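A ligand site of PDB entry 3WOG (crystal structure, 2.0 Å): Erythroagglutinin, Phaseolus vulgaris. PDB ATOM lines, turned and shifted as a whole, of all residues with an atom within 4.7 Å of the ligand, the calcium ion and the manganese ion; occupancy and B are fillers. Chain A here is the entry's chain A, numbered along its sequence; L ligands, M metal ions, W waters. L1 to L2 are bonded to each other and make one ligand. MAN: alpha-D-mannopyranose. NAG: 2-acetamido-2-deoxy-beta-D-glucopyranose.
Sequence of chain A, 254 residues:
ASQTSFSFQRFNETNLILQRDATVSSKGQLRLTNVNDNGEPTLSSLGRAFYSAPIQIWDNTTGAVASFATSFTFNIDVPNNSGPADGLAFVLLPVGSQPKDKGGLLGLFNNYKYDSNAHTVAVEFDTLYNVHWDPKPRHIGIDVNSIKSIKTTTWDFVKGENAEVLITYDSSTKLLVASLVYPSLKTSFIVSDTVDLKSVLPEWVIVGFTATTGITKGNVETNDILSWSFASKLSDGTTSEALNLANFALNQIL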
ATOM      1  N   ASP A  86      -1.532  30.446  14.545  1.00  0.00           N
ATOM      2  CA  ASP A  86      -2.791  30.918  15.159  1.00  0.00           C
ATOM      3  C   ASP A  86      -2.753  32.385  15.594  1.00  0.00           C
ATOM      4  O   ASP A  86      -3.781  33.042  15.731  1.00  0.00           O
ATOM      5  CB  ASP A  86      -3.114  30.063  16.365  1.00  0.00           C
ATOM      6  CG  ASP A  86      -3.995  28.906  16.015  1.00  0.00           C
ATOM      7  OD1 ASP A  86      -5.197  29.145  15.735  1.00  0.00           O
ATOM      8  OD2 ASP A  86      -3.470  27.762  16.002  1.00  0.00           O
ATOM      9  N   LYS A 102      -1.999  24.703  23.263  1.00  0.00           N
ATOM     10  CA  LYS A 102      -1.484  25.284  22.031  1.00  0.00           C
ATOM     11  C   LYS A 102      -2.616  25.703  21.049  1.00  0.00           C
ATOM     12  O   LYS A 102      -3.779  25.842  21.455  1.00  0.00           O
ATOM     13  CB  LYS A 102      -0.503  24.307  21.382  1.00  0.00           C
ATOM     14  CG  LYS A 102      -1.111  22.938  21.104  1.00  0.00           C
ATOM     15  CD  LYS A 102      -0.162  22.070  20.282  1.00  0.00           C
ATOM     16  CE  LYS A 102       0.981  21.512  21.124  1.00  0.00           C
ATOM     17  NZ  LYS A 102       2.040  20.864  20.291  1.00  0.00           N
ATOM     18  N   GLY A 103      -2.276  25.938  19.783  1.00  0.00           N
ATOM     19  CA  GLY A 103      -3.278  26.310  18.779  1.00  0.00           C
ATOM     20  C   GLY A 103      -4.031  27.577  19.113  1.00  0.00           C
ATOM     21  O   GLY A 103      -3.439  28.571  19.541  1.00  0.00           O
ATOM     22  N   GLY A 104      -5.349  27.560  18.927  1.00  0.00           N
ATOM     23  CA  GLY A 104      -6.163  28.756  19.127  1.00  0.00           C
ATOM     24  C   GLY A 104      -6.249  29.267  20.558  1.00  0.00           C
ATOM     25  O   GLY A 104      -6.758  30.350  20.797  1.00  0.00           O
ATOM     26  N   LEU A 105      -5.788  28.489  21.526  1.00  0.00           N
ATOM     27  CA  LEU A 105      -5.750  28.947  22.917  1.00  0.00           C
ATOM     28  C   LEU A 105      -4.477  29.746  23.245  1.00  0.00           C
ATOM     29  O   LEU A 105      -4.299  30.248  24.370  1.00  0.00           O
ATOM     30  CB  LEU A 105      -5.942  27.743  23.856  1.00  0.00           C
ATOM     31  CG  LEU A 105      -7.302  27.052  23.658  1.00  0.00           C
ATOM     32  CD1 LEU A 105      -7.442  25.766  24.490  1.00  0.00           C
ATOM     33  CD2 LEU A 105      -8.451  27.990  23.951  1.00  0.00           C
ATOM     34  N   TYR A 112     -12.120  27.319  26.329  1.00  0.00           N
ATOM     35  CA  TYR A 112     -12.619  28.632  25.976  1.00  0.00           C
ATOM     36  C   TYR A 112     -13.625  29.269  26.918  1.00  0.00           C
ATOM     37  O   TYR A 112     -14.279  30.248  26.565  1.00  0.00           O
ATOM     38  CB  TYR A 112     -13.106  28.711  24.526  1.00  0.00           C
ATOM     39  CG  TYR A 112     -14.103  27.666  24.071  1.00  0.00           C
ATOM     40  CD1 TYR A 112     -15.478  27.949  24.015  1.00  0.00           C
ATOM     41  CD2 TYR A 112     -13.673  26.405  23.633  1.00  0.00           C
ATOM     42  CE1 TYR A 112     -16.390  27.000  23.566  1.00  0.00           C
ATOM     43  CE2 TYR A 112     -14.568  25.453  23.169  1.00  0.00           C
ATOM     44  CZ  TYR A 112     -15.914  25.749  23.144  1.00  0.00           C
ATOM     45  OH  TYR A 112     -16.789  24.788  22.678  1.00  0.00           O
ATOM     46  N   GLU A 124      -4.188  40.214  21.902  1.00  0.00           N
ATOM     47  CA  GLU A 124      -3.951  39.192  20.896  1.00  0.00           C
ATOM     48  C   GLU A 124      -4.002  39.739  19.481  1.00  0.00           C
ATOM     49  O   GLU A 124      -4.757  40.671  19.174  1.00  0.00           O
ATOM     50  CB  GLU A 124      -4.993  38.046  21.019  1.00  0.00           C
ATOM     51  CG  GLU A 124      -6.453  38.422  20.789  1.00  0.00           C
ATOM     52  CD  GLU A 124      -7.361  37.197  20.659  1.00  0.00           C
ATOM     53  OE1 GLU A 124      -7.216  36.274  21.508  1.00  0.00           O
ATOM     54  OE2 GLU A 124      -8.174  37.112  19.685  1.00  0.00           O
ATOM     55  N   ASP A 126      -4.804  37.851  16.313  1.00  0.00           N
ATOM     56  CA  ASP A 126      -5.387  36.511  16.083  1.00  0.00           C
ATOM     57  C   ASP A 126      -5.576  36.348  14.576  1.00  0.00           C
ATOM     58  O   ASP A 126      -6.322  37.101  13.945  1.00  0.00           O
ATOM     59  CB  ASP A 126      -6.753  36.419  16.853  1.00  0.00           C
ATOM     60  CG  ASP A 126      -7.361  35.014  16.852  1.00  0.00           C
ATOM     61  OD1 ASP A 126      -6.931  34.212  16.007  1.00  0.00           O
ATOM     62  OD2 ASP A 126      -8.294  34.730  17.704  1.00  0.00           O
ATOM     63  N   LEU A 128      -6.473  33.422  12.988  1.00  0.00           N
ATOM     64  CA  LEU A 128      -7.315  32.297  12.593  1.00  0.00           C
ATOM     65  C   LEU A 128      -8.632  32.282  13.353  1.00  0.00           C
ATOM     66  O   LEU A 128      -8.658  32.261  14.592  1.00  0.00           O
ATOM     67  CB  LEU A 128      -6.561  30.979  12.784  1.00  0.00           C
ATOM     68  CG  LEU A 128      -7.410  29.771  12.332  1.00  0.00           C
ATOM     69  CD1 LEU A 128      -6.684  28.945  11.287  1.00  0.00           C
ATOM     70  CD2 LEU A 128      -7.969  28.936  13.480  1.00  0.00           C
ATOM     71  N   TYR A 129      -9.721  32.307  12.576  1.00  0.00           N
ATOM     72  CA  TYR A 129     -11.079  32.208  13.093  1.00  0.00           C
ATOM     73  C   TYR A 129     -11.362  30.875  13.796  1.00  0.00           C
ATOM     74  O   TYR A 129     -11.329  29.803  13.188  1.00  0.00           O
ATOM     75  CB  TYR A 129     -12.072  32.427  11.942  1.00  0.00           C
ATOM     76  CG  TYR A 129     -13.536  32.076  12.205  1.00  0.00           C
ATOM     77  CD1 TYR A 129     -14.282  32.781  13.145  1.00  0.00           C
ATOM     78  CD2 TYR A 129     -14.171  31.080  11.460  1.00  0.00           C
ATOM     79  CE1 TYR A 129     -15.634  32.491  13.364  1.00  0.00           C
ATOM     80  CE2 TYR A 129     -15.508  30.764  11.661  1.00  0.00           C
ATOM     81  CZ  TYR A 129     -16.241  31.472  12.607  1.00  0.00           C
ATOM     82  OH  TYR A 129     -17.561  31.176  12.797  1.00  0.00           O
ATOM     83  N   ASN A 130     -11.644  30.951  15.088  1.00  0.00           N
ATOM     84  CA  ASN A 130     -12.002  29.779  15.855  1.00  0.00           C
ATOM     85  C   ASN A 130     -13.493  29.855  16.106  1.00  0.00           C
ATOM     86  O   ASN A 130     -13.963  30.738  16.857  1.00  0.00           O
ATOM     87  CB  ASN A 130     -11.222  29.740  17.170  1.00  0.00           C
ATOM     88  CG  ASN A 130      -9.766  29.392  16.972  1.00  0.00           C
ATOM     89  OD1 ASN A 130      -8.885  30.275  17.001  1.00  0.00           O
ATOM     90  ND2 ASN A 130      -9.483  28.109  16.740  1.00  0.00           N
ATOM     91  N   VAL A 131     -14.239  28.959  15.446  1.00  0.00           N
ATOM     92  CA  VAL A 131     -15.707  29.043  15.389  1.00  0.00           C
ATOM     93  C   VAL A 131     -16.420  29.210  16.743  1.00  0.00           C
ATOM     94  O   VAL A 131     -17.459  29.886  16.844  1.00  0.00           O
ATOM     95  CB  VAL A 131     -16.294  27.813  14.625  1.00  0.00           C
ATOM     96  CG1 VAL A 131     -15.995  26.507  15.355  1.00  0.00           C
ATOM     97  CG2 VAL A 131     -17.782  27.977  14.402  1.00  0.00           C
ATOM     98  N   HIS A 132     -15.892  28.594  17.799  1.00  0.00           N
ATOM     99  CA  HIS A 132     -16.581  28.616  19.087  1.00  0.00           C
ATOM    100  C   HIS A 132     -16.425  29.915  19.845  1.00  0.00           C
ATOM    101  O   HIS A 132     -17.094  30.112  20.856  1.00  0.00           O
ATOM    102  CB  HIS A 132     -16.166  27.454  19.963  1.00  0.00           C
ATOM    103  CG  HIS A 132     -16.529  26.098  19.387  1.00  0.00           C
ATOM    104  ND1 HIS A 132     -17.763  25.807  18.920  1.00  0.00           N
ATOM    105  CD2 HIS A 132     -15.771  24.936  19.246  1.00  0.00           C
ATOM    106  CE1 HIS A 132     -17.793  24.530  18.481  1.00  0.00           C
ATOM    107  NE2 HIS A 132     -16.561  23.993  18.681  1.00  0.00           N
ATOM    108  N   TRP A 133     -15.553  30.830  19.392  1.00  0.00           N
ATOM    109  CA  TRP A 133     -15.432  32.100  20.137  1.00  0.00           C
ATOM    110  C   TRP A 133     -15.006  33.326  19.385  1.00  0.00           C
ATOM    111  O   TRP A 133     -15.244  34.431  19.866  1.00  0.00           O
ATOM    112  CB  TRP A 133     -14.534  31.934  21.352  1.00  0.00           C
ATOM    113  CG  TRP A 133     -13.101  31.643  20.975  1.00  0.00           C
ATOM    114  CD1 TRP A 133     -12.124  32.549  20.559  1.00  0.00           C
ATOM    115  CD2 TRP A 133     -12.453  30.338  20.950  1.00  0.00           C
ATOM    116  NE1 TRP A 133     -10.936  31.899  20.295  1.00  0.00           N
ATOM    117  CE2 TRP A 133     -11.063  30.571  20.509  1.00  0.00           C
ATOM    118  CE3 TRP A 133     -12.847  29.031  21.248  1.00  0.00           C
ATOM    119  CZ2 TRP A 133     -10.156  29.533  20.379  1.00  0.00           C
ATOM    120  CZ3 TRP A 133     -11.909  27.997  21.118  1.00  0.00           C
ATOM    121  CH2 TRP A 133     -10.604  28.251  20.705  1.00  0.00           C
ATOM    122  N   ASP A 134     -14.337  33.179  18.235  1.00  0.00           N
ATOM    123  CA  ASP A 134     -13.772  34.349  17.528  1.00  0.00           C
ATOM    124  C   ASP A 134     -14.780  35.079  16.652  1.00  0.00           C
ATOM    125  O   ASP A 134     -15.709  34.449  16.117  1.00  0.00           O
ATOM    126  CB  ASP A 134     -12.621  33.919  16.623  1.00  0.00           C
ATOM    127  CG  ASP A 134     -11.274  33.832  17.356  1.00  0.00           C
ATOM    128  OD1 ASP A 134     -10.947  34.647  18.291  1.00  0.00           O
ATOM    129  OD2 ASP A 134     -10.518  32.928  16.936  1.00  0.00           O
ATOM    130  N   HIS A 139      -8.325  39.768  13.654  1.00  0.00           N
ATOM    131  CA  HIS A 139      -8.699  40.765  14.655  1.00  0.00           C
ATOM    132  C   HIS A 139      -7.616  41.048  15.665  1.00  0.00           C
ATOM    133  O   HIS A 139      -6.780  40.196  15.931  1.00  0.00           O
ATOM    134  CB  HIS A 139     -10.006  40.335  15.373  1.00  0.00           C
ATOM    135  CG  HIS A 139      -9.950  38.945  16.019  1.00  0.00           C
ATOM    136  ND1 HIS A 139     -10.210  37.819  15.340  1.00  0.00           N
ATOM    137  CD2 HIS A 139      -9.706  38.560  17.352  1.00  0.00           C
ATOM    138  CE1 HIS A 139     -10.106  36.753  16.153  1.00  0.00           C
ATOM    139  NE2 HIS A 139      -9.798  37.203  17.401  1.00  0.00           N
ATOM    140  N   ILE A 147      -9.968  33.319  26.348  1.00  0.00           N
ATOM    141  CA  ILE A 147      -9.634  33.395  24.920  1.00  0.00           C
ATOM    142  C   ILE A 147     -10.725  34.150  24.148  1.00  0.00           C
ATOM    143  O   ILE A 147     -10.514  34.616  23.014  1.00  0.00           O
ATOM    144  CB  ILE A 147      -9.376  31.980  24.323  1.00  0.00           C
ATOM    145  CG1 ILE A 147      -8.516  32.032  23.046  1.00  0.00           C
ATOM    146  CG2 ILE A 147     -10.692  31.241  24.063  1.00  0.00           C
ATOM    147  CD1 ILE A 147      -7.192  32.768  23.194  1.00  0.00           C
ATOM    148  N   SER A 149     -12.273  37.300  23.571  1.00  0.00           N
ATOM    149  CA  SER A 149     -11.900  38.693  23.834  1.00  0.00           C
ATOM    150  C   SER A 149     -13.066  39.522  24.347  1.00  0.00           C
ATOM    151  O   SER A 149     -14.207  39.368  23.881  1.00  0.00           O
ATOM    152  CB  SER A 149     -11.307  39.351  22.584  1.00  0.00           C
ATOM    153  OG  SER A 149     -10.305  38.517  22.011  1.00  0.00           O
ATOM    154  N   GLY A 214      -0.654  26.767  13.745  1.00  0.00           N
ATOM    155  CA  GLY A 214      -1.829  25.891  13.603  1.00  0.00           C
ATOM    156  C   GLY A 214      -1.485  24.444  13.885  1.00  0.00           C
ATOM    157  O   GLY A 214      -0.342  24.012  13.721  1.00  0.00           O
ATOM    158  N   ILE A 215      -2.473  23.686  14.339  1.00  0.00           N
ATOM    159  CA  ILE A 215      -2.274  22.266  14.522  1.00  0.00           C
ATOM    160  C   ILE A 215      -2.545  21.484  13.217  1.00  0.00           C
ATOM    161  O   ILE A 215      -2.010  20.389  13.030  1.00  0.00           O
ATOM    162  CB  ILE A 215      -3.031  21.689  15.747  1.00  0.00           C
ATOM    163  CG1 ILE A 215      -4.549  21.669  15.522  1.00  0.00           C
ATOM    164  CG2 ILE A 215      -2.686  22.467  17.020  1.00  0.00           C
ATOM    165  CD1 ILE A 215      -5.266  20.673  16.421  1.00  0.00           C
ATOM    166  N   THR A 216      -3.340  22.048  12.315  1.00  0.00           N
ATOM    167  CA  THR A 216      -3.774  21.373  11.097  1.00  0.00           C
ATOM    168  C   THR A 216      -2.980  21.843   9.888  1.00  0.00           C
ATOM    169  O   THR A 216      -2.886  23.037   9.632  1.00  0.00           O
ATOM    170  CB  THR A 216      -5.282  21.587  10.840  1.00  0.00           C
ATOM    171  OG1 THR A 216      -6.016  21.099  11.971  1.00  0.00           O
ATOM    172  CG2 THR A 216      -5.761  20.830   9.610  1.00  0.00           C
ATOM    173  N   ASN A 219      -2.287  25.520   7.916  1.00  0.00           N
ATOM    174  CA  ASN A 219      -2.541  26.659   8.798  1.00  0.00           C
ATOM    175  C   ASN A 219      -1.301  26.902   9.666  1.00  0.00           C
ATOM    176  O   ASN A 219      -1.080  26.195  10.636  1.00  0.00           O
ATOM    177  CB  ASN A 219      -3.771  26.383   9.670  1.00  0.00           C
ATOM    178  CG  ASN A 219      -5.007  26.071   8.848  1.00  0.00           C
ATOM    179  OD1 ASN A 219      -5.709  26.974   8.404  1.00  0.00           O
ATOM    180  ND2 ASN A 219      -5.285  24.787   8.662  1.00  0.00           N
HETATM  181  C1  MAN L   1      -9.151  22.629  17.462  1.00  0.00           C
HETATM  182  C2  MAN L   1      -8.086  23.611  16.960  1.00  0.00           C
HETATM  183  C3  MAN L   1      -7.352  24.250  18.135  1.00  0.00           C
HETATM  184  C4  MAN L   1      -8.372  24.966  19.031  1.00  0.00           C
HETATM  185  C5  MAN L   1      -9.437  23.961  19.464  1.00  0.00           C
HETATM  186  C6  MAN L   1     -10.587  24.602  20.239  1.00  0.00           C
HETATM  187  O1  MAN L   1      -8.582  21.509  18.123  1.00  0.00           O
HETATM  188  O2  MAN L   1      -8.720  24.659  16.257  1.00  0.00           O
HETATM  189  O3  MAN L   1      -6.402  25.178  17.631  1.00  0.00           O
HETATM  190  O4  MAN L   1      -7.753  25.591  20.135  1.00  0.00           O
HETATM  191  O5  MAN L   1     -10.030  23.311  18.340  1.00  0.00           O
HETATM  192  O6  MAN L   1     -11.131  23.607  21.087  1.00  0.00           O
HETATM  193  C1  NAG L   2      -8.786  24.403  14.846  1.00  0.00           C
HETATM  194  C2  NAG L   2     -10.085  25.006  14.321  1.00  0.00           C
HETATM  195  C3  NAG L   2     -10.221  24.891  12.782  1.00  0.00           C
HETATM  196  C4  NAG L   2      -8.918  25.318  12.088  1.00  0.00           C
HETATM  197  C5  NAG L   2      -7.685  24.654  12.741  1.00  0.00           C
HETATM  198  C6  NAG L   2      -6.370  25.161  12.159  1.00  0.00           C
HETATM  199  C7  NAG L   2     -11.926  24.964  15.910  1.00  0.00           C
HETATM  200  C8  NAG L   2     -13.022  24.108  16.486  1.00  0.00           C
HETATM  201  N2  NAG L   2     -11.175  24.350  14.990  1.00  0.00           N
HETATM  202  O3  NAG L   2     -11.298  25.680  12.302  1.00  0.00           O
HETATM  203  O4  NAG L   2      -9.021  25.052  10.692  1.00  0.00           O
HETATM  204  O5  NAG L   2      -7.662  24.894  14.149  1.00  0.00           O
HETATM  205  O6  NAG L   2      -5.277  24.455  12.726  1.00  0.00           O
HETATM  206  O7  NAG L   2     -11.777  26.150  16.258  1.00  0.00           O
HETATM  207 CA    CA M   1      -8.240  32.496  16.898  1.00  0.00          CA
HETATM  208 MN    MN M   2      -9.468  35.873  18.825  1.00  0.00          MN
HETATM  209  O   HOH W   1      -6.889  27.198  16.007  1.00  0.00           O
HETATM  210  O   HOH W   2      -8.115  32.341  19.232  1.00  0.00           O
HETATM  211  O   HOH W   3     -12.968  27.517  13.246  1.00  0.00           O
HETATM  212  O   HOH W   4     -10.753  36.838  19.921  1.00  0.00           O
HETATM  213  O   HOH W   5     -13.418  27.193  18.225  1.00  0.00           O
HETATM  214  O   HOH W   6      -9.161  34.765  20.387  1.00  0.00           O
HETATM  215  O   HOH W   7      -6.162  31.505  16.569  1.00  0.00           O
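The side-chain amide nitrogen (ND2) of Asn 130 sits at hydrogen-bond distance from an oxygen (O7) of NAG L2, at 3.1 Å. N of Gly 104 lies within hydrogen-bond range of O3 of MAN L1, 2.9 Å away. The backbone NH (N) of Thr 216 is in hydrogen-bond range of an oxygen (O6) of NAG L2. The backbone NH (N) of Ile 215 sits at hydrogen-bond distance from an oxygen (O6) of NAG L2 (3.3 Å).
OG of Ser 149 sits close to OE2 of Glu 124, at 3.5 Å. OD1 of Asp 134 sits close to NE1 of Trp 133 (3.4 Å). The side-chain carboxylate of Asp 86 is in hydrogen-bond range of the backbone NH of Gly 104 (3.5 Å). The side-chain amide nitrogen (ND2) of Asn 219 sits at hydrogen-bond distance from the backbone carbonyl oxygen (O) of Thr 216. The backbone carbonyl oxygen of Asn 219 sits close to the backbone NH of Gly 214, at 3.2 Å.
CA of Gly 103 touches O3 of MAN L1, 3.5 Å away. N of Leu 105 touches O4 of MAN L1 (3.8 Å). N of Val 131 touches O7 of NAG L2, 3.8 Å away. His 132 touches the ligand. Trp 133 touches the ligand. CA of Gly 214 touches O6 of NAG L2, 3.8 Å away. ND2 of Asn 219 touches C6 of NAG L2, 3.7 Å away. Hydrophobic or aromatic side chains within 4 Å of the ligand: Leu 105, Leu 128, Val 131, His 132, Trp 133 and Ile 215. The nearest printed residue that does not touch the ligand is Lys 102 (4.2 Å).
The nearest printed residue that does not touch the calcium ion is Trp 133 (4.4 Å).
Within 4 Å of the manganese ion: Glu 124, Asp 126, Asp 134 and His 139. The nearest printed residue that does not touch the manganese ion is Ser 149 (4.2 Å).
OD1 of Asn 130 binds the calcium ion (2.3 Å). The calcium ion is bound by OD2 of Asp 134, at 2.3 Å. Water W7 binds the calcium ion, 2.3 Å away. OD1 of Asp 126 is bound to the calcium ion (2.3 Å). The calcium ion is bound by water W2, at 2.3 Å. The calcium ion is bound by the backbone carbonyl oxygen (O) of Leu 128. The side-chain carboxylate (OD2) of Asp 126 is bound to the calcium ion, at 2.4 Å. The calcium ion has seven donor atoms within binding distance.
The manganese ion is bound by water W6, water W4, NE2 of His 139, OD2 of Asp 126, OE2 of Glu 124 and OD1 of Asp 134. The manganese ion has six donor atoms within binding distance.
Water W2 bridges O of Gly 104 (2.9 Å) and NE1 of Trp 133 (3.0 Å). Water W6 lies within hydrogen-bond range of OE1 of Glu 124 (2.7 Å), O of Ile 147 (3.0 Å) and NE1 of Trp 133 (3.4 Å). Water W1 lies within hydrogen-bond range of the side-chain carboxylate (OD1) of Asp 86 (2.6 Å), an oxygen (O3) of MAN L1 (2.6 Å), the side-chain amide nitrogen (ND2) of Asn 130 (2.8 Å) and the backbone NH (N) of Gly 104 (3.3 Å). Water W3 lies within hydrogen-bond range of an oxygen (O3) of NAG L2 (2.7 Å), the backbone carbonyl oxygen (O) of Tyr 129 (2.8 Å) and the backbone NH (N) of Val 131 (2.9 Å). Water W5 lies within hydrogen-bond range of an oxygen (O7) of NAG L2, the backbone NH (N) of His 132 and the backbone NH (N) of Val 131.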
